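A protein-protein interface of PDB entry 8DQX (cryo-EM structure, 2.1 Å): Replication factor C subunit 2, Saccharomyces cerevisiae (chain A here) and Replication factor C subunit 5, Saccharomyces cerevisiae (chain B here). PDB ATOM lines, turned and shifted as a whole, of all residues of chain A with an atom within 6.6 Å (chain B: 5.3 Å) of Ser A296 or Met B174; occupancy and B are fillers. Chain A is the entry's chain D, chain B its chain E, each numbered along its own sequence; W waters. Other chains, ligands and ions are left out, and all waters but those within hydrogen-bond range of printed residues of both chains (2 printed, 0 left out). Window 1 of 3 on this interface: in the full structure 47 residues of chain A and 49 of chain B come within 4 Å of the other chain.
The backbone NH (N) of Ala A297 lies within hydrogen-bond range of the side-chain carboxylate (OE2) of Glu A339, 3.0 Å away. The backbone carbonyl oxygen (O) of Ser A296 is in hydrogen-bond range of the side-chain hydroxyl (OG) of Ser A299. The side-chain sulfur (SG) of Cys B171 sits at hydrogen-bond distance from the backbone carbonyl oxygen (O) of Ser B173 (3.3 Å). The side-chain amino group of Lys B182 is in hydrogen-bond range of the backbone carbonyl oxygen of Met B174, at 3.5 Å.
Among the printed residues, pairs that only touch across the chains: Glu A339 with Ser B173 (3.0 Å), Gly A294 with Tyr B42 (3.1 Å) and Ser A296 with Met B174 (3.7 Å).
Of the printed residues of chain B, Gly A294 touches Tyr B42. Printed residues of chain B within 4 Å of Glu A339: Ser B173 (3.0 Å). Printed residues of chain A within 4 Å of Tyr B42: Gly A294. Of the printed residues of chain A, Ser B173 touches Glu A339. Printed residues of chain A within 4 Å of Met B174: Ser A296. The nearest printed residue of chain A that does not touch Met B174 is Glu A339 (4.01 Å).
Of the 12 printed residues of chain A, 3 touch a printed residue of chain B. Along chain A the printed residues that touch a printed residue of chain B span positions 294 to 339. Hydrophobic or aromatic side chains of chain B that line the printed part of chain A: Tyr B42 and Met B174. Among the printed residues, 3 pairs touch across the chains.
Water W2 lies within hydrogen-bond range of the backbone carbonyl oxygen (O) of Gly A261 (2.8 Å), the side-chain hydroxyl (OH) of Tyr B42 (3.0 Å) and the backbone NH (N) of Ser A296 (3.0 Å). Water W1 lies within hydrogen-bond range of the backbone NH (N) of Met B174 and the side-chain carboxylate (OE2) of Glu A339.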
ATOM      1  N   GLY A 261     -16.302 -19.656   3.245  1.00  0.00           N
ATOM      2  CA  GLY A 261     -15.290 -18.627   3.099  1.00  0.00           C
ATOM      3  C   GLY A 261     -13.871 -19.119   3.283  1.00  0.00           C
ATOM      4  O   GLY A 261     -13.008 -18.350   3.712  1.00  0.00           O
ATOM      5  N   VAL A 263     -10.254 -20.221   1.879  1.00  0.00           N
ATOM      6  CA  VAL A 263      -9.457 -19.848   0.705  1.00  0.00           C
ATOM      7  C   VAL A 263      -9.109 -21.106  -0.089  1.00  0.00           C
ATOM      8  O   VAL A 263      -8.645 -22.094   0.503  1.00  0.00           O
ATOM      9  CB  VAL A 263      -8.194 -19.103   1.139  1.00  0.00           C
ATOM     10  CG1 VAL A 263      -7.344 -18.734  -0.066  1.00  0.00           C
ATOM     11  CG2 VAL A 263      -8.566 -17.860   1.935  1.00  0.00           C
ATOM     12  N   PHE A 290      -5.208  -9.665  -3.781  1.00  0.00           N
ATOM     13  CA  PHE A 290      -5.895 -10.685  -2.996  1.00  0.00           C
ATOM     14  C   PHE A 290      -7.022 -10.087  -2.160  1.00  0.00           C
ATOM     15  O   PHE A 290      -8.089 -10.693  -2.024  1.00  0.00           O
ATOM     16  CB  PHE A 290      -4.869 -11.399  -2.110  1.00  0.00           C
ATOM     17  CG  PHE A 290      -5.457 -12.363  -1.122  1.00  0.00           C
ATOM     18  CD1 PHE A 290      -5.646 -13.694  -1.458  1.00  0.00           C
ATOM     19  CD2 PHE A 290      -5.790 -11.949   0.159  1.00  0.00           C
ATOM     20  CE1 PHE A 290      -6.172 -14.585  -0.543  1.00  0.00           C
ATOM     21  CE2 PHE A 290      -6.319 -12.834   1.076  1.00  0.00           C
ATOM     22  CZ  PHE A 290      -6.508 -14.155   0.727  1.00  0.00           C
ATOM     23  N   GLY A 294     -12.225 -10.292  -0.880  1.00  0.00           N
ATOM     24  CA  GLY A 294     -12.997 -10.254   0.345  1.00  0.00           C
ATOM     25  C   GLY A 294     -12.714 -11.366   1.330  1.00  0.00           C
ATOM     26  O   GLY A 294     -13.443 -11.490   2.319  1.00  0.00           O
ATOM     27  N   TRP A 295     -11.680 -12.172   1.099  1.00  0.00           N
ATOM     28  CA  TRP A 295     -11.305 -13.218   2.040  1.00  0.00           C
ATOM     29  C   TRP A 295     -11.113 -12.644   3.438  1.00  0.00           C
ATOM     30  O   TRP A 295     -10.449 -11.622   3.618  1.00  0.00           O
ATOM     31  CB  TRP A 295     -10.010 -13.892   1.578  1.00  0.00           C
ATOM     32  CG  TRP A 295     -10.078 -14.491   0.211  1.00  0.00           C
ATOM     33  CD1 TRP A 295      -9.340 -14.134  -0.878  1.00  0.00           C
ATOM     34  CD2 TRP A 295     -10.925 -15.560  -0.212  1.00  0.00           C
ATOM     35  NE1 TRP A 295      -9.674 -14.916  -1.955  1.00  0.00           N
ATOM     36  CE2 TRP A 295     -10.649 -15.800  -1.571  1.00  0.00           C
ATOM     37  CE3 TRP A 295     -11.893 -16.338   0.428  1.00  0.00           C
ATOM     38  CZ2 TRP A 295     -11.302 -16.784  -2.301  1.00  0.00           C
ATOM     39  CZ3 TRP A 295     -12.542 -17.312  -0.297  1.00  0.00           C
ATOM     40  CH2 TRP A 295     -12.245 -17.527  -1.648  1.00  0.00           C
ATOM     41  N   SER A 296     -11.696 -13.308   4.430  1.00  0.00           N
ATOM     42  CA  SER A 296     -11.504 -12.892   5.812  1.00  0.00           C
ATOM     43  C   SER A 296     -10.069 -13.171   6.241  1.00  0.00           C
ATOM     44  O   SER A 296      -9.560 -14.280   6.060  1.00  0.00           O
ATOM     45  CB  SER A 296     -12.484 -13.623   6.728  1.00  0.00           C
ATOM     46  OG  SER A 296     -12.183 -13.377   8.087  1.00  0.00           O
ATOM     47  N   ALA A 297      -9.412 -12.158   6.812  1.00  0.00           N
ATOM     48  CA  ALA A 297      -8.004 -12.314   7.169  1.00  0.00           C
ATOM     49  C   ALA A 297      -7.808 -13.394   8.226  1.00  0.00           C
ATOM     50  O   ALA A 297      -6.783 -14.084   8.221  1.00  0.00           O
ATOM     51  CB  ALA A 297      -7.434 -10.981   7.654  1.00  0.00           C
ATOM     52  N   ALA A 298      -8.768 -13.557   9.136  1.00  0.00           N
ATOM     53  CA  ALA A 298      -8.631 -14.564  10.183  1.00  0.00           C
ATOM     54  C   ALA A 298      -8.581 -15.970   9.597  1.00  0.00           C
ATOM     55  O   ALA A 298      -7.768 -16.799  10.021  1.00  0.00           O
ATOM     56  CB  ALA A 298      -9.780 -14.436  11.183  1.00  0.00           C
ATOM     57  N   SER A 299      -9.438 -16.255   8.614  1.00  0.00           N
ATOM     58  CA  SER A 299      -9.401 -17.558   7.959  1.00  0.00           C
ATOM     59  C   SER A 299      -8.080 -17.762   7.225  1.00  0.00           C
ATOM     60  O   SER A 299      -7.508 -18.859   7.248  1.00  0.00           O
ATOM     61  CB  SER A 299     -10.589 -17.699   7.004  1.00  0.00           C
ATOM     62  OG  SER A 299     -10.177 -17.650   5.651  1.00  0.00           O
ATOM     63  N   VAL A 300      -7.571 -16.708   6.583  1.00  0.00           N
ATOM     64  CA  VAL A 300      -6.291 -16.800   5.886  1.00  0.00           C
ATOM     65  C   VAL A 300      -5.176 -17.143   6.869  1.00  0.00           C
ATOM     66  O   VAL A 300      -4.332 -18.007   6.604  1.00  0.00           O
ATOM     67  CB  VAL A 300      -5.995 -15.485   5.138  1.00  0.00           C
ATOM     68  CG1 VAL A 300      -4.625 -15.537   4.490  1.00  0.00           C
ATOM     69  CG2 VAL A 300      -7.066 -15.203   4.095  1.00  0.00           C
ATOM     70  N   VAL A 301      -5.153 -16.464   8.017  1.00  0.00           N
ATOM     71  CA  VAL A 301      -4.111 -16.721   9.007  1.00  0.00           C
ATOM     72  C   VAL A 301      -4.236 -18.139   9.549  1.00  0.00           C
ATOM     73  O   VAL A 301      -3.233 -18.831   9.747  1.00  0.00           O
ATOM     74  CB  VAL A 301      -4.164 -15.672  10.136  1.00  0.00           C
ATOM     75  CG1 VAL A 301      -3.254 -16.075  11.282  1.00  0.00           C
ATOM     76  CG2 VAL A 301      -3.776 -14.291   9.612  1.00  0.00           C
ATOM     77  N   GLU A 339      -7.507  -5.288   8.138  1.00  0.00           N
ATOM     78  CA  GLU A 339      -7.058  -6.616   7.726  1.00  0.00           C
ATOM     79  C   GLU A 339      -5.924  -6.545   6.706  1.00  0.00           C
ATOM     80  O   GLU A 339      -4.987  -7.347   6.759  1.00  0.00           O
ATOM     81  CB  GLU A 339      -8.238  -7.408   7.163  1.00  0.00           C
ATOM     82  CG  GLU A 339      -9.215  -7.896   8.228  1.00  0.00           C
ATOM     83  CD  GLU A 339     -10.529  -8.378   7.639  1.00  0.00           C
ATOM     84  OE1 GLU A 339     -11.369  -7.527   7.279  1.00  0.00           O
ATOM     85  OE2 GLU A 339     -10.720  -9.607   7.530  1.00  0.00           O
ATOM     86  N   LEU B  40     -25.086 -11.828   7.139  1.00  0.00           N
ATOM     87  CA  LEU B  40     -24.007 -10.861   7.321  1.00  0.00           C
ATOM     88  C   LEU B  40     -23.216 -10.789   6.021  1.00  0.00           C
ATOM     89  O   LEU B  40     -22.478 -11.720   5.692  1.00  0.00           O
ATOM     90  CB  LEU B  40     -23.105 -11.247   8.496  1.00  0.00           C
ATOM     91  CG  LEU B  40     -21.831 -10.417   8.720  1.00  0.00           C
ATOM     92  CD1 LEU B  40     -22.061  -8.933   8.491  1.00  0.00           C
ATOM     93  CD2 LEU B  40     -21.293 -10.652  10.122  1.00  0.00           C
ATOM     94  N   TYR B  42     -20.239  -9.263   3.804  1.00  0.00           N
ATOM     95  CA  TYR B  42     -18.938  -8.643   4.008  1.00  0.00           C
ATOM     96  C   TYR B  42     -18.164  -8.621   2.697  1.00  0.00           C
ATOM     97  O   TYR B  42     -18.353  -9.475   1.829  1.00  0.00           O
ATOM     98  CB  TYR B  42     -18.135  -9.356   5.112  1.00  0.00           C
ATOM     99  CG  TYR B  42     -17.679 -10.762   4.782  1.00  0.00           C
ATOM    100  CD1 TYR B  42     -18.527 -11.847   4.956  1.00  0.00           C
ATOM    101  CD2 TYR B  42     -16.393 -11.003   4.316  1.00  0.00           C
ATOM    102  CE1 TYR B  42     -18.114 -13.131   4.665  1.00  0.00           C
ATOM    103  CE2 TYR B  42     -15.969 -12.281   4.021  1.00  0.00           C
ATOM    104  CZ  TYR B  42     -16.831 -13.344   4.197  1.00  0.00           C
ATOM    105  OH  TYR B  42     -16.409 -14.617   3.908  1.00  0.00           O
ATOM    106  N   CYS B 171     -21.185  -5.095   6.380  1.00  0.00           N
ATOM    107  CA  CYS B 171     -19.936  -4.546   6.885  1.00  0.00           C
ATOM    108  C   CYS B 171     -18.846  -4.704   5.836  1.00  0.00           C
ATOM    109  O   CYS B 171     -18.916  -5.573   4.966  1.00  0.00           O
ATOM    110  CB  CYS B 171     -19.525  -5.220   8.200  1.00  0.00           C
ATOM    111  SG  CYS B 171     -18.908  -6.901   8.028  1.00  0.00           S
ATOM    112  N   ASP B 172     -17.835  -3.840   5.924  1.00  0.00           N
ATOM    113  CA  ASP B 172     -16.684  -3.940   5.037  1.00  0.00           C
ATOM    114  C   ASP B 172     -15.573  -4.814   5.606  1.00  0.00           C
ATOM    115  O   ASP B 172     -14.675  -5.211   4.856  1.00  0.00           O
ATOM    116  CB  ASP B 172     -16.137  -2.545   4.716  1.00  0.00           C
ATOM    117  CG  ASP B 172     -15.495  -1.880   5.914  1.00  0.00           C
ATOM    118  OD1 ASP B 172     -14.314  -1.494   5.820  1.00  0.00           O
ATOM    119  OD2 ASP B 172     -16.172  -1.747   6.953  1.00  0.00           O
ATOM    120  N   SER B 173     -15.610  -5.126   6.900  1.00  0.00           N
ATOM    121  CA  SER B 173     -14.663  -6.052   7.507  1.00  0.00           C
ATOM    122  C   SER B 173     -15.322  -6.723   8.701  1.00  0.00           C
ATOM    123  O   SER B 173     -16.085  -6.088   9.432  1.00  0.00           O
ATOM    124  CB  SER B 173     -13.377  -5.348   7.958  1.00  0.00           C
ATOM    125  OG  SER B 173     -13.660  -4.092   8.548  1.00  0.00           O
ATOM    126  N   MET B 174     -15.008  -7.998   8.903  1.00  0.00           N
ATOM    127  CA  MET B 174     -15.544  -8.755  10.026  1.00  0.00           C
ATOM    128  C   MET B 174     -14.640  -8.723  11.250  1.00  0.00           C
ATOM    129  O   MET B 174     -15.028  -9.246  12.299  1.00  0.00           O
ATOM    130  CB  MET B 174     -15.792 -10.204   9.607  1.00  0.00           C
ATOM    131  CG  MET B 174     -17.169 -10.427   8.999  1.00  0.00           C
ATOM    132  SD  MET B 174     -17.501 -12.100   8.413  1.00  0.00           S
ATOM    133  CE  MET B 174     -15.860 -12.741   8.089  1.00  0.00           C
ATOM    134  N   SER B 175     -13.462  -8.115  11.145  1.00  0.00           N
ATOM    135  CA  SER B 175     -12.533  -8.084  12.270  1.00  0.00           C
ATOM    136  C   SER B 175     -13.153  -7.534  13.552  1.00  0.00           C
ATOM    137  O   SER B 175     -12.899  -8.113  14.620  1.00  0.00           O
ATOM    138  CB  SER B 175     -11.287  -7.277  11.867  1.00  0.00           C
ATOM    139  OG  SER B 175     -10.409  -7.094  12.960  1.00  0.00           O
ATOM    140  N   PRO B 176     -13.947  -6.464  13.538  1.00  0.00           N
ATOM    141  CA  PRO B 176     -14.547  -5.968  14.785  1.00  0.00           C
ATOM    142  C   PRO B 176     -15.861  -6.629  15.184  1.00  0.00           C
ATOM    143  O   PRO B 176     -16.438  -6.227  16.199  1.00  0.00           O
ATOM    144  CB  PRO B 176     -14.765  -4.469  14.486  1.00  0.00           C
ATOM    145  CG  PRO B 176     -14.152  -4.218  13.118  1.00  0.00           C
ATOM    146  CD  PRO B 176     -14.188  -5.529  12.429  1.00  0.00           C
ATOM    147  N   ILE B 177     -16.341  -7.622  14.440  1.00  0.00           N
ATOM    148  CA  ILE B 177     -17.567  -8.331  14.797  1.00  0.00           C
ATOM    149  C   ILE B 177     -17.225  -9.406  15.824  1.00  0.00           C
ATOM    150  O   ILE B 177     -16.379 -10.268  15.572  1.00  0.00           O
ATOM    151  CB  ILE B 177     -18.235  -8.946  13.557  1.00  0.00           C
ATOM    152  CG1 ILE B 177     -18.495  -7.887  12.475  1.00  0.00           C
ATOM    153  CG2 ILE B 177     -19.531  -9.641  13.948  1.00  0.00           C
ATOM    154  CD1 ILE B 177     -19.581  -6.895  12.820  1.00  0.00           C
ATOM    155  N   LYS B 182     -21.086 -13.451  14.793  1.00  0.00           N
ATOM    156  CA  LYS B 182     -20.768 -14.185  13.574  1.00  0.00           C
ATOM    157  C   LYS B 182     -21.296 -15.610  13.646  1.00  0.00           C
ATOM    158  O   LYS B 182     -21.775 -16.154  12.646  1.00  0.00           O
ATOM    159  CB  LYS B 182     -19.259 -14.177  13.330  1.00  0.00           C
ATOM    160  CG  LYS B 182     -18.795 -13.008  12.484  1.00  0.00           C
ATOM    161  CD  LYS B 182     -17.544 -12.365  13.029  1.00  0.00           C
ATOM    162  CE  LYS B 182     -16.386 -13.333  13.096  1.00  0.00           C
ATOM    163  NZ  LYS B 182     -15.102 -12.603  13.231  1.00  0.00           N
ATOM    164  N   LEU B 187     -22.776 -16.042   6.712  1.00  0.00           N
ATOM    165  CA  LEU B 187     -21.788 -15.080   6.235  1.00  0.00           C
ATOM    166  C   LEU B 187     -21.697 -15.146   4.715  1.00  0.00           C
ATOM    167  O   LEU B 187     -21.439 -16.214   4.152  1.00  0.00           O
ATOM    168  CB  LEU B 187     -20.423 -15.353   6.867  1.00  0.00           C
ATOM    169  CG  LEU B 187     -20.421 -15.670   8.365  1.00  0.00           C
ATOM    170  CD1 LEU B 187     -19.011 -15.993   8.848  1.00  0.00           C
ATOM    171  CD2 LEU B 187     -21.016 -14.525   9.162  1.00  0.00           C
HETATM  172  O   HOH W   1     -13.669  -9.519   6.765  1.00  0.00           O
HETATM  173  O   HOH W   2     -13.626 -15.599   3.957  1.00  0.00           O
